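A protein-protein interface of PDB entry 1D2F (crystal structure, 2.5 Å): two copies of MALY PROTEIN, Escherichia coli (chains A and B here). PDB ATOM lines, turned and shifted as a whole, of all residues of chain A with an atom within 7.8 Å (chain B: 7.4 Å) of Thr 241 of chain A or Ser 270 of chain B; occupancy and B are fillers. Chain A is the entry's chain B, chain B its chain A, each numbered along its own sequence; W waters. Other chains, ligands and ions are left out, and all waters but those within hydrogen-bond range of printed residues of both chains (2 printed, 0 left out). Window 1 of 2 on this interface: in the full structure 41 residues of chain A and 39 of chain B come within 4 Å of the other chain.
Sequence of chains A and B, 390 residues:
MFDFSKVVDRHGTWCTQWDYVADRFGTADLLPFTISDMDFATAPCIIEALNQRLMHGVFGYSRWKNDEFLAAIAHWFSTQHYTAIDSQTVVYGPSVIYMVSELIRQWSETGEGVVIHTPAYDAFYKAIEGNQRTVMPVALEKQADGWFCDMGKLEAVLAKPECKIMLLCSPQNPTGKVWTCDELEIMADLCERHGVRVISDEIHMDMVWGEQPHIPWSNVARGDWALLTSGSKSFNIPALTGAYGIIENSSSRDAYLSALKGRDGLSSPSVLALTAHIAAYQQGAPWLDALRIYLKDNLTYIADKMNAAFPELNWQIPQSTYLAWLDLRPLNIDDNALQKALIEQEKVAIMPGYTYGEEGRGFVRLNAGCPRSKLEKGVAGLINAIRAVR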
ATOM      1  N   TYR A  92      37.363  14.774  13.437  1.00  0.00           N
ATOM      2  CA  TYR A  92      35.936  14.894  13.711  1.00  0.00           C
ATOM      3  C   TYR A  92      35.726  15.854  14.872  1.00  0.00           C
ATOM      4  O   TYR A  92      36.642  16.089  15.671  1.00  0.00           O
ATOM      5  CB  TYR A  92      35.378  13.518  14.081  1.00  0.00           C
ATOM      6  CG  TYR A  92      33.977  13.529  14.631  1.00  0.00           C
ATOM      7  CD1 TYR A  92      32.874  13.573  13.787  1.00  0.00           C
ATOM      8  CD2 TYR A  92      33.752  13.532  16.008  1.00  0.00           C
ATOM      9  CE1 TYR A  92      31.577  13.621  14.300  1.00  0.00           C
ATOM     10  CE2 TYR A  92      32.462  13.582  16.533  1.00  0.00           C
ATOM     11  CZ  TYR A  92      31.377  13.624  15.668  1.00  0.00           C
ATOM     12  OH  TYR A  92      30.088  13.648  16.173  1.00  0.00           O
ATOM     13  N   GLY A  93      34.521  16.414  14.957  1.00  0.00           N
ATOM     14  CA  GLY A  93      34.181  17.311  16.045  1.00  0.00           C
ATOM     15  C   GLY A  93      32.688  17.211  16.311  1.00  0.00           C
ATOM     16  O   GLY A  93      31.948  16.807  15.428  1.00  0.00           O
ATOM     17  N   PRO A  94      32.210  17.533  17.518  1.00  0.00           N
ATOM     18  CA  PRO A  94      30.774  17.466  17.824  1.00  0.00           C
ATOM     19  C   PRO A  94      30.027  18.575  17.072  1.00  0.00           C
ATOM     20  O   PRO A  94      28.887  18.397  16.641  1.00  0.00           O
ATOM     21  CB  PRO A  94      30.724  17.703  19.323  1.00  0.00           C
ATOM     22  CG  PRO A  94      32.060  17.257  19.790  1.00  0.00           C
ATOM     23  CD  PRO A  94      32.995  17.746  18.743  1.00  0.00           C
ATOM     24  N   SER A  95      30.684  19.722  16.924  1.00  0.00           N
ATOM     25  CA  SER A  95      30.092  20.860  16.238  1.00  0.00           C
ATOM     26  C   SER A  95      31.232  21.747  15.804  1.00  0.00           C
ATOM     27  O   SER A  95      32.334  21.616  16.316  1.00  0.00           O
ATOM     28  CB  SER A  95      29.186  21.652  17.189  1.00  0.00           C
ATOM     29  OG  SER A  95      29.961  22.349  18.156  1.00  0.00           O
ATOM     30  N   SER A 230      31.076  21.235   7.831  1.00  0.00           N
ATOM     31  CA  SER A 230      30.101  20.202   8.091  1.00  0.00           C
ATOM     32  C   SER A 230      29.105  20.278   6.944  1.00  0.00           C
ATOM     33  O   SER A 230      29.161  21.195   6.145  1.00  0.00           O
ATOM     34  CB  SER A 230      29.399  20.497   9.416  1.00  0.00           C
ATOM     35  OG  SER A 230      28.104  19.948   9.425  1.00  0.00           O
ATOM     36  N   GLY A 231      28.207  19.310   6.859  1.00  0.00           N
ATOM     37  CA  GLY A 231      27.198  19.346   5.827  1.00  0.00           C
ATOM     38  C   GLY A 231      25.888  19.775   6.454  1.00  0.00           C
ATOM     39  O   GLY A 231      24.849  19.795   5.796  1.00  0.00           O
ATOM     40  N   SER A 232      25.925  20.140   7.734  1.00  0.00           N
ATOM     41  CA  SER A 232      24.694  20.536   8.428  1.00  0.00           C
ATOM     42  C   SER A 232      23.969  21.750   7.834  1.00  0.00           C
ATOM     43  O   SER A 232      22.745  21.769   7.798  1.00  0.00           O
ATOM     44  CB  SER A 232      24.961  20.775   9.914  1.00  0.00           C
ATOM     45  OG  SER A 232      25.792  21.897  10.121  1.00  0.00           O
ATOM     46  N   ILE A 237      20.834  19.252   8.246  1.00  0.00           N
ATOM     47  CA  ILE A 237      20.845  18.130   9.184  1.00  0.00           C
ATOM     48  C   ILE A 237      21.550  18.488  10.494  1.00  0.00           C
ATOM     49  O   ILE A 237      22.182  17.639  11.120  1.00  0.00           O
ATOM     50  CB  ILE A 237      21.552  16.892   8.591  1.00  0.00           C
ATOM     51  CG1 ILE A 237      22.948  17.274   8.098  1.00  0.00           C
ATOM     52  CG2 ILE A 237      20.735  16.320   7.464  1.00  0.00           C
ATOM     53  CD1 ILE A 237      23.742  16.108   7.527  1.00  0.00           C
ATOM     54  N   PRO A 238      21.433  19.746  10.947  1.00  0.00           N
ATOM     55  CA  PRO A 238      22.121  20.063  12.199  1.00  0.00           C
ATOM     56  C   PRO A 238      21.693  19.199  13.383  1.00  0.00           C
ATOM     57  O   PRO A 238      22.502  18.918  14.275  1.00  0.00           O
ATOM     58  CB  PRO A 238      21.807  21.550  12.401  1.00  0.00           C
ATOM     59  CG  PRO A 238      20.464  21.694  11.805  1.00  0.00           C
ATOM     60  CD  PRO A 238      20.557  20.856  10.532  1.00  0.00           C
ATOM     61  N   ALA A 239      20.432  18.767  13.389  1.00  0.00           N
ATOM     62  CA  ALA A 239      19.910  17.939  14.490  1.00  0.00           C
ATOM     63  C   ALA A 239      20.558  16.555  14.574  1.00  0.00           C
ATOM     64  O   ALA A 239      20.187  15.744  15.420  1.00  0.00           O
ATOM     65  CB  ALA A 239      18.398  17.784  14.365  1.00  0.00           C
ATOM     66  N   LEU A 240      21.508  16.277  13.690  1.00  0.00           N
ATOM     67  CA  LEU A 240      22.202  14.999  13.695  1.00  0.00           C
ATOM     68  C   LEU A 240      23.570  15.188  14.356  1.00  0.00           C
ATOM     69  O   LEU A 240      24.239  14.216  14.718  1.00  0.00           O
ATOM     70  CB  LEU A 240      22.392  14.512  12.258  1.00  0.00           C
ATOM     71  CG  LEU A 240      21.507  13.390  11.712  1.00  0.00           C
ATOM     72  CD1 LEU A 240      20.088  13.593  12.169  1.00  0.00           C
ATOM     73  CD2 LEU A 240      21.598  13.350  10.184  1.00  0.00           C
ATOM     74  N   THR A 241      23.956  16.453  14.525  1.00  0.00           N
ATOM     75  CA  THR A 241      25.249  16.846  15.091  1.00  0.00           C
ATOM     76  C   THR A 241      26.375  16.354  14.187  1.00  0.00           C
ATOM     77  O   THR A 241      26.131  15.697  13.169  1.00  0.00           O
ATOM     78  CB  THR A 241      25.511  16.291  16.528  1.00  0.00           C
ATOM     79  OG1 THR A 241      25.771  14.888  16.473  1.00  0.00           O
ATOM     80  CG2 THR A 241      24.325  16.551  17.430  1.00  0.00           C
ATOM     81  N   GLY A 242      27.604  16.687  14.564  1.00  0.00           N
ATOM     82  CA  GLY A 242      28.760  16.283  13.792  1.00  0.00           C
ATOM     83  C   GLY A 242      29.312  17.400  12.932  1.00  0.00           C
ATOM     84  O   GLY A 242      28.582  18.260  12.433  1.00  0.00           O
ATOM     85  N   ALA A 243      30.626  17.395  12.766  1.00  0.00           N
ATOM     86  CA  ALA A 243      31.303  18.378  11.944  1.00  0.00           C
ATOM     87  C   ALA A 243      32.650  17.728  11.726  1.00  0.00           C
ATOM     88  O   ALA A 243      32.923  16.686  12.326  1.00  0.00           O
ATOM     89  CB  ALA A 243      31.449  19.694  12.693  1.00  0.00           C
ATOM     90  N   SER A 268      33.746   9.547  20.618  1.00  0.00           N
ATOM     91  CA  SER A 268      32.719   8.668  20.064  1.00  0.00           C
ATOM     92  C   SER A 268      31.685   9.529  19.327  1.00  0.00           C
ATOM     93  O   SER A 268      30.961  10.310  19.942  1.00  0.00           O
ATOM     94  CB  SER A 268      32.053   7.879  21.191  1.00  0.00           C
ATOM     95  OG  SER A 268      30.918   7.174  20.712  1.00  0.00           O
ATOM     96  N   PRO A 269      31.595   9.386  17.998  1.00  0.00           N
ATOM     97  CA  PRO A 269      30.662  10.161  17.179  1.00  0.00           C
ATOM     98  C   PRO A 269      29.295   9.535  17.019  1.00  0.00           C
ATOM     99  O   PRO A 269      29.113   8.355  17.281  1.00  0.00           O
ATOM    100  CB  PRO A 269      31.374  10.210  15.847  1.00  0.00           C
ATOM    101  CG  PRO A 269      31.844   8.783  15.745  1.00  0.00           C
ATOM    102  CD  PRO A 269      32.429   8.527  17.137  1.00  0.00           C
ATOM    103  N   SER A 270      28.329  10.333  16.580  1.00  0.00           N
ATOM    104  CA  SER A 270      27.014   9.784  16.329  1.00  0.00           C
ATOM    105  C   SER A 270      27.183   9.140  14.961  1.00  0.00           C
ATOM    106  O   SER A 270      27.468   9.810  13.959  1.00  0.00           O
ATOM    107  CB  SER A 270      25.940  10.873  16.281  1.00  0.00           C
ATOM    108  OG  SER A 270      26.233  11.832  15.296  1.00  0.00           O
ATOM    109  N   VAL A 271      27.048   7.819  14.947  1.00  0.00           N
ATOM    110  CA  VAL A 271      27.188   7.032  13.735  1.00  0.00           C
ATOM    111  C   VAL A 271      26.259   7.539  12.628  1.00  0.00           C
ATOM    112  O   VAL A 271      26.582   7.416  11.445  1.00  0.00           O
ATOM    113  CB  VAL A 271      26.900   5.524  14.026  1.00  0.00           C
ATOM    114  CG1 VAL A 271      25.414   5.295  14.241  1.00  0.00           C
ATOM    115  CG2 VAL A 271      27.421   4.670  12.899  1.00  0.00           C
ATOM    116  N   LEU A 272      25.113   8.106  12.999  1.00  0.00           N
ATOM    117  CA  LEU A 272      24.182   8.603  11.991  1.00  0.00           C
ATOM    118  C   LEU A 272      24.656   9.888  11.324  1.00  0.00           C
ATOM    119  O   LEU A 272      24.322  10.141  10.170  1.00  0.00           O
ATOM    120  CB  LEU A 272      22.789   8.793  12.585  1.00  0.00           C
ATOM    121  CG  LEU A 272      22.135   7.468  12.994  1.00  0.00           C
ATOM    122  CD1 LEU A 272      20.766   7.722  13.610  1.00  0.00           C
ATOM    123  CD2 LEU A 272      22.004   6.573  11.776  1.00  0.00           C
ATOM    124  N   ALA A 273      25.435  10.691  12.038  1.00  0.00           N
ATOM    125  CA  ALA A 273      25.964  11.915  11.463  1.00  0.00           C
ATOM    126  C   ALA A 273      26.953  11.510  10.367  1.00  0.00           C
ATOM    127  O   ALA A 273      26.984  12.110   9.306  1.00  0.00           O
ATOM    128  CB  ALA A 273      26.661  12.757  12.528  1.00  0.00           C
ATOM    129  N   LEU A 274      27.757  10.485  10.630  1.00  0.00           N
ATOM    130  CA  LEU A 274      28.711   9.995   9.645  1.00  0.00           C
ATOM    131  C   LEU A 274      27.970   9.465   8.430  1.00  0.00           C
ATOM    132  O   LEU A 274      28.306   9.796   7.301  1.00  0.00           O
ATOM    133  CB  LEU A 274      29.569   8.868  10.221  1.00  0.00           C
ATOM    134  CG  LEU A 274      30.515   9.218  11.370  1.00  0.00           C
ATOM    135  CD1 LEU A 274      31.338   7.986  11.725  1.00  0.00           C
ATOM    136  CD2 LEU A 274      31.424  10.369  10.976  1.00  0.00           C
ATOM    137  N   ALA A 276      24.971  10.166   7.328  1.00  0.00           N
ATOM    138  CA  ALA A 276      24.332  11.246   6.573  1.00  0.00           C
ATOM    139  C   ALA A 276      25.346  11.957   5.675  1.00  0.00           C
ATOM    140  O   ALA A 276      25.053  12.256   4.520  1.00  0.00           O
ATOM    141  CB  ALA A 276      23.695  12.250   7.518  1.00  0.00           C
ATOM    142  N   HIS A 277      26.538  12.223   6.193  1.00  0.00           N
ATOM    143  CA  HIS A 277      27.549  12.893   5.384  1.00  0.00           C
ATOM    144  C   HIS A 277      27.994  12.033   4.203  1.00  0.00           C
ATOM    145  O   HIS A 277      28.132  12.524   3.080  1.00  0.00           O
ATOM    146  CB  HIS A 277      28.763  13.279   6.233  1.00  0.00           C
ATOM    147  CG  HIS A 277      28.573  14.544   7.007  1.00  0.00           C
ATOM    148  ND1 HIS A 277      27.762  14.623   8.119  1.00  0.00           N
ATOM    149  CD2 HIS A 277      29.047  15.797   6.797  1.00  0.00           C
ATOM    150  CE1 HIS A 277      27.740  15.869   8.556  1.00  0.00           C
ATOM    151  NE2 HIS A 277      28.511  16.603   7.772  1.00  0.00           N
ATOM    152  N   PHE B  59      15.476  17.849   9.719  1.00  0.00           N
ATOM    153  CA  PHE B  59      16.450  17.694  10.797  1.00  0.00           C
ATOM    154  C   PHE B  59      17.052  19.008  11.238  1.00  0.00           C
ATOM    155  O   PHE B  59      18.256  19.100  11.470  1.00  0.00           O
ATOM    156  CB  PHE B  59      17.565  16.730  10.379  1.00  0.00           C
ATOM    157  CG  PHE B  59      17.107  15.303  10.230  1.00  0.00           C
ATOM    158  CD1 PHE B  59      16.823  14.775   8.976  1.00  0.00           C
ATOM    159  CD2 PHE B  59      16.925  14.497  11.352  1.00  0.00           C
ATOM    160  CE1 PHE B  59      16.361  13.456   8.840  1.00  0.00           C
ATOM    161  CE2 PHE B  59      16.467  13.181  11.231  1.00  0.00           C
ATOM    162  CZ  PHE B  59      16.183  12.662   9.974  1.00  0.00           C
ATOM    163  N   SER B  62      16.877  21.503  17.151  1.00  0.00           N
ATOM    164  CA  SER B  62      15.900  21.065  18.136  1.00  0.00           C
ATOM    165  C   SER B  62      16.394  21.413  19.535  1.00  0.00           C
ATOM    166  O   SER B  62      17.600  21.527  19.762  1.00  0.00           O
ATOM    167  CB  SER B  62      15.687  19.561  18.025  1.00  0.00           C
ATOM    168  OG  SER B  62      15.311  19.217  16.704  1.00  0.00           O
ATOM    169  N   TRP B  64      16.645  20.576  23.684  1.00  0.00           N
ATOM    170  CA  TRP B  64      16.665  19.413  24.563  1.00  0.00           C
ATOM    171  C   TRP B  64      15.703  19.646  25.723  1.00  0.00           C
ATOM    172  O   TRP B  64      15.268  18.695  26.375  1.00  0.00           O
ATOM    173  CB  TRP B  64      18.071  19.137  25.104  1.00  0.00           C
ATOM    174  CG  TRP B  64      18.638  20.239  25.927  1.00  0.00           C
ATOM    175  CD1 TRP B  64      19.459  21.244  25.502  1.00  0.00           C
ATOM    176  CD2 TRP B  64      18.413  20.468  27.323  1.00  0.00           C
ATOM    177  NE1 TRP B  64      19.760  22.086  26.546  1.00  0.00           N
ATOM    178  CE2 TRP B  64      19.131  21.633  27.676  1.00  0.00           C
ATOM    179  CE3 TRP B  64      17.673  19.800  28.312  1.00  0.00           C
ATOM    180  CZ2 TRP B  64      19.133  22.147  28.981  1.00  0.00           C
ATOM    181  CZ3 TRP B  64      17.675  20.310  29.608  1.00  0.00           C
ATOM    182  CH2 TRP B  64      18.402  21.475  29.929  1.00  0.00           C
ATOM    183  N   TYR B  92      21.206  18.482  29.766  1.00  0.00           N
ATOM    184  CA  TYR B  92      21.673  17.589  28.707  1.00  0.00           C
ATOM    185  C   TYR B  92      23.184  17.700  28.567  1.00  0.00           C
ATOM    186  O   TYR B  92      23.776  18.722  28.920  1.00  0.00           O
ATOM    187  CB  TYR B  92      21.020  17.982  27.379  1.00  0.00           C
ATOM    188  CG  TYR B  92      21.634  17.321  26.171  1.00  0.00           C
ATOM    189  CD1 TYR B  92      21.226  16.054  25.768  1.00  0.00           C
ATOM    190  CD2 TYR B  92      22.636  17.955  25.439  1.00  0.00           C
ATOM    191  CE1 TYR B  92      21.794  15.424  24.659  1.00  0.00           C
ATOM    192  CE2 TYR B  92      23.218  17.336  24.324  1.00  0.00           C
ATOM    193  CZ  TYR B  92      22.789  16.067  23.937  1.00  0.00           C
ATOM    194  OH  TYR B  92      23.340  15.453  22.823  1.00  0.00           O
ATOM    195  N   PRO B  94      26.660  16.011  25.908  1.00  0.00           N
ATOM    196  CA  PRO B  94      27.035  15.203  24.735  1.00  0.00           C
ATOM    197  C   PRO B  94      27.400  13.789  25.163  1.00  0.00           C
ATOM    198  O   PRO B  94      27.139  12.824  24.452  1.00  0.00           O
ATOM    199  CB  PRO B  94      28.257  15.926  24.173  1.00  0.00           C
ATOM    200  CG  PRO B  94      28.119  17.330  24.688  1.00  0.00           C
ATOM    201  CD  PRO B  94      27.594  17.135  26.084  1.00  0.00           C
ATOM    202  N   ALA B 239      26.304   4.882  20.203  1.00  0.00           N
ATOM    203  CA  ALA B 239      26.551   5.469  18.891  1.00  0.00           C
ATOM    204  C   ALA B 239      25.543   6.559  18.528  1.00  0.00           C
ATOM    205  O   ALA B 239      25.618   7.128  17.442  1.00  0.00           O
ATOM    206  CB  ALA B 239      26.541   4.385  17.823  1.00  0.00           C
ATOM    207  N   LEU B 240      24.599   6.831  19.426  1.00  0.00           N
ATOM    208  CA  LEU B 240      23.599   7.872  19.202  1.00  0.00           C
ATOM    209  C   LEU B 240      23.989   9.138  19.972  1.00  0.00           C
ATOM    210  O   LEU B 240      23.422  10.211  19.758  1.00  0.00           O
ATOM    211  CB  LEU B 240      22.227   7.394  19.687  1.00  0.00           C
ATOM    212  CG  LEU B 240      21.169   6.950  18.669  1.00  0.00           C
ATOM    213  CD1 LEU B 240      21.760   6.086  17.595  1.00  0.00           C
ATOM    214  CD2 LEU B 240      20.082   6.187  19.401  1.00  0.00           C
ATOM    215  N   THR B 241      24.969   8.990  20.861  1.00  0.00           N
ATOM    216  CA  THR B 241      25.459  10.058  21.731  1.00  0.00           C
ATOM    217  C   THR B 241      24.333  10.537  22.650  1.00  0.00           C
ATOM    218  O   THR B 241      23.197  10.068  22.563  1.00  0.00           O
ATOM    219  CB  THR B 241      26.033  11.304  20.955  1.00  0.00           C
ATOM    220  OG1 THR B 241      24.964  12.061  20.372  1.00  0.00           O
ATOM    221  CG2 THR B 241      27.005  10.871  19.864  1.00  0.00           C
ATOM    222  N   GLY B 242      24.661  11.471  23.534  1.00  0.00           N
ATOM    223  CA  GLY B 242      23.666  11.988  24.443  1.00  0.00           C
ATOM    224  C   GLY B 242      23.806  11.404  25.831  1.00  0.00           C
ATOM    225  O   GLY B 242      24.225  10.259  26.024  1.00  0.00           O
ATOM    226  N   LEU B 266      27.763  23.438  22.248  1.00  0.00           N
ATOM    227  CA  LEU B 266      27.235  22.070  22.200  1.00  0.00           C
ATOM    228  C   LEU B 266      25.790  21.941  22.703  1.00  0.00           C
ATOM    229  O   LEU B 266      25.329  20.821  22.972  1.00  0.00           O
ATOM    230  CB  LEU B 266      28.103  21.142  23.054  1.00  0.00           C
ATOM    231  CG  LEU B 266      29.580  20.952  22.731  1.00  0.00           C
ATOM    232  CD1 LEU B 266      30.304  20.401  23.946  1.00  0.00           C
ATOM    233  CD2 LEU B 266      29.717  20.037  21.539  1.00  0.00           C
ATOM    234  N   SER B 267      25.071  23.053  22.829  1.00  0.00           N
ATOM    235  CA  SER B 267      23.701  22.992  23.347  1.00  0.00           C
ATOM    236  C   SER B 267      22.704  22.298  22.408  1.00  0.00           C
ATOM    237  O   SER B 267      21.674  21.782  22.855  1.00  0.00           O
ATOM    238  CB  SER B 267      23.200  24.394  23.690  1.00  0.00           C
ATOM    239  OG  SER B 267      23.029  25.173  22.518  1.00  0.00           O
ATOM    240  N   SER B 268      22.994  22.293  21.112  1.00  0.00           N
ATOM    241  CA  SER B 268      22.120  21.631  20.150  1.00  0.00           C
ATOM    242  C   SER B 268      22.362  20.121  20.234  1.00  0.00           C
ATOM    243  O   SER B 268      23.430  19.638  19.867  1.00  0.00           O
ATOM    244  CB  SER B 268      22.429  22.124  18.748  1.00  0.00           C
ATOM    245  OG  SER B 268      21.764  21.322  17.794  1.00  0.00           O
ATOM    246  N   PRO B 269      21.362  19.356  20.696  1.00  0.00           N
ATOM    247  CA  PRO B 269      21.457  17.899  20.845  1.00  0.00           C
ATOM    248  C   PRO B 269      21.085  17.105  19.612  1.00  0.00           C
ATOM    249  O   PRO B 269      20.453  17.625  18.694  1.00  0.00           O
ATOM    250  CB  PRO B 269      20.472  17.626  21.960  1.00  0.00           C
ATOM    251  CG  PRO B 269      19.333  18.501  21.529  1.00  0.00           C
ATOM    252  CD  PRO B 269      20.036  19.823  21.139  1.00  0.00           C
ATOM    253  N   SER B 270      21.472  15.836  19.589  1.00  0.00           N
ATOM    254  CA  SER B 270      21.092  15.001  18.468  1.00  0.00           C
ATOM    255  C   SER B 270      19.647  14.611  18.783  1.00  0.00           C
ATOM    256  O   SER B 270      19.363  13.933  19.777  1.00  0.00           O
ATOM    257  CB  SER B 270      21.984  13.762  18.362  1.00  0.00           C
ATOM    258  OG  SER B 270      21.983  13.023  19.556  1.00  0.00           O
ATOM    259  N   VAL B 271      18.736  15.082  17.945  1.00  0.00           N
ATOM    260  CA  VAL B 271      17.332  14.808  18.128  1.00  0.00           C
ATOM    261  C   VAL B 271      17.044  13.310  18.249  1.00  0.00           C
ATOM    262  O   VAL B 271      16.089  12.917  18.895  1.00  0.00           O
ATOM    263  CB  VAL B 271      16.511  15.402  16.957  1.00  0.00           C
ATOM    264  CG1 VAL B 271      16.675  14.554  15.712  1.00  0.00           C
ATOM    265  CG2 VAL B 271      15.065  15.515  17.349  1.00  0.00           C
ATOM    266  N   LEU B 272      17.874  12.474  17.635  1.00  0.00           N
ATOM    267  CA  LEU B 272      17.637  11.037  17.693  1.00  0.00           C
ATOM    268  C   LEU B 272      18.006  10.438  19.039  1.00  0.00           C
ATOM    269  O   LEU B 272      17.426   9.427  19.452  1.00  0.00           O
ATOM    270  CB  LEU B 272      18.372  10.310  16.561  1.00  0.00           C
ATOM    271  CG  LEU B 272      17.809  10.615  15.164  1.00  0.00           C
ATOM    272  CD1 LEU B 272      18.569   9.845  14.104  1.00  0.00           C
ATOM    273  CD2 LEU B 272      16.348  10.248  15.118  1.00  0.00           C
ATOM    274  N   ALA B 273      18.961  11.054  19.727  1.00  0.00           N
ATOM    275  CA  ALA B 273      19.339  10.558  21.044  1.00  0.00           C
ATOM    276  C   ALA B 273      18.149  10.805  21.979  1.00  0.00           C
ATOM    277  O   ALA B 273      17.813   9.960  22.805  1.00  0.00           O
ATOM    278  CB  ALA B 273      20.579  11.278  21.555  1.00  0.00           C
ATOM    279  N   LEU B 274      17.500  11.957  21.835  1.00  0.00           N
ATOM    280  CA  LEU B 274      16.352  12.277  22.666  1.00  0.00           C
ATOM    281  C   LEU B 274      15.234  11.288  22.374  1.00  0.00           C
ATOM    282  O   LEU B 274      14.637  10.716  23.291  1.00  0.00           O
ATOM    283  CB  LEU B 274      15.853  13.694  22.388  1.00  0.00           C
ATOM    284  CG  LEU B 274      16.767  14.872  22.742  1.00  0.00           C
ATOM    285  CD1 LEU B 274      16.021  16.167  22.473  1.00  0.00           C
ATOM    286  CD2 LEU B 274      17.195  14.808  24.199  1.00  0.00           C
ATOM    287  N   THR B 275      14.952  11.087  21.097  1.00  0.00           N
ATOM    288  CA  THR B 275      13.904  10.167  20.688  1.00  0.00           C
ATOM    289  C   THR B 275      14.141   8.760  21.237  1.00  0.00           C
ATOM    290  O   THR B 275      13.210   8.104  21.712  1.00  0.00           O
ATOM    291  CB  THR B 275      13.807  10.089  19.154  1.00  0.00           C
ATOM    292  OG1 THR B 275      13.396  11.360  18.640  1.00  0.00           O
ATOM    293  CG2 THR B 275      12.808   9.035  18.735  1.00  0.00           C
ATOM    294  N   ALA B 276      15.387   8.299  21.168  1.00  0.00           N
ATOM    295  CA  ALA B 276      15.731   6.971  21.648  1.00  0.00           C
ATOM    296  C   ALA B 276      15.455   6.850  23.145  1.00  0.00           C
ATOM    297  O   ALA B 276      14.894   5.852  23.594  1.00  0.00           O
ATOM    298  CB  ALA B 276      17.193   6.672  21.350  1.00  0.00           C
HETATM  299  O   HOH W   1      29.261  11.232  22.527  1.00  0.00           O
HETATM  300  O   HOH W   2      20.150  12.773  16.196  1.00  0.00           O
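Of the printed residues of chain B, Thr 241 of chain A touches Pro 269 (3.9 Å) and Ser 270 (3.6 Å).
Printed residues of chain B within 4 Å of Val 271 of chain A: Ala 239 (3.0 Å).
Ala 273 of chain A touches none of the printed residues of chain B.
Printed residues of chain A within 4 Å of Phe 59 of chain B: Ile 237, Pro 238, Ala 239 and Leu 240.
Trp 64 of chain B touches none of the printed residues of chain A.
The nearest residue of chain B that does not touch Thr 241 of chain A is Ser 268 of chain B (4.03 Å).
The nearest residue of chain A that does not touch Ser 270 of chain B is Leu 240 of chain A (4.3 Å).
Water W2 lies within hydrogen-bond range of N of Leu 272 of chain B (2.7 Å), O of Ala 239 of chain A (3.1 Å) and N of Val 271 of chain B (3.2 Å).
Water W1 lies within hydrogen-bond range of O of Ser 268 of chain A (3.2 Å) and O of Pro 94 of chain B (3.3 Å).
Ala 239 of chain A touches Val 271 of chain B, and with the chains exchanged Val 271 of chain A touches Ala 239 of chain B.
Thr 241 of chain A touches Ser 270 of chain B, and with the chains exchanged Ser 270 of chain A touches Thr 241 of chain B.
Leu 272 of chain B touches its own counterpart, Leu 272 of chain A.
Positions printed for both chains: 92, 94, 239, 240, 241, 242, 268, 269, 270, 271, 272, 273, 274 and 276.
Among the printed residues, merely in contact across the chains: Leu 272 of chain A with Leu 272 of chain B, Ser 270 of chain A with Ala 239 of chain B, Ala 239 of chain A with Ser 270 of chain B, Pro 94 of chain A with Leu 266 of chain B, Leu 240 of chain A with Phe 59 of chain B, Ile 237 of chain A with Phe 59 of chain B, Ser 270 of chain A with Thr 241 of chain B, Thr 241 of chain A with Ser 270 of chain B, Pro 269 of chain A with Ala 239 of chain B, Ala 239 of chain A with Pro 269 of chain B, Pro 269 of chain A with Thr 241 of chain B, Thr 241 of chain A with Pro 269 of chain B and Ser 268 of chain A with Thr 241 of chain B.
N of Ala 239 of chain A is in hydrogen-bond range of O of Phe 59 of chain B.
O of Ala 239 of chain B is in hydrogen-bond range of N of Val 271 of chain A (3.0 Å).
The backbone NH of Val 271 of chain B is in hydrogen-bond range of the backbone carbonyl oxygen of Ala 239 of chain A (3.0 Å).
The backbone nitrogen of Pro 238 of chain A lies close to the backbone carbonyl oxygen of Phe 59 of chain B (3.3 Å).
Of the 23 printed residues of chain A, 11 touch a printed residue of chain B.
Hydrophobic or aromatic side chains of chain A within 4 Å of the printed part of chain B: Pro 94, Pro 238, Ala 239, Leu 240, Val 271 and Leu 272.
The backbone NH (N) of Gly 242 of chain A is in hydrogen-bond range of the backbone carbonyl oxygen (O) of Pro 94 of chain A, 3.0 Å away.
The backbone NH of Ile 237 of chain A lies within hydrogen-bond range of the backbone carbonyl oxygen of Ser 232 of chain A (3.2 Å).
OG of Ser 270 of chain A lies within hydrogen-bond range of O of Leu 240 of chain A, 3.2 Å away.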
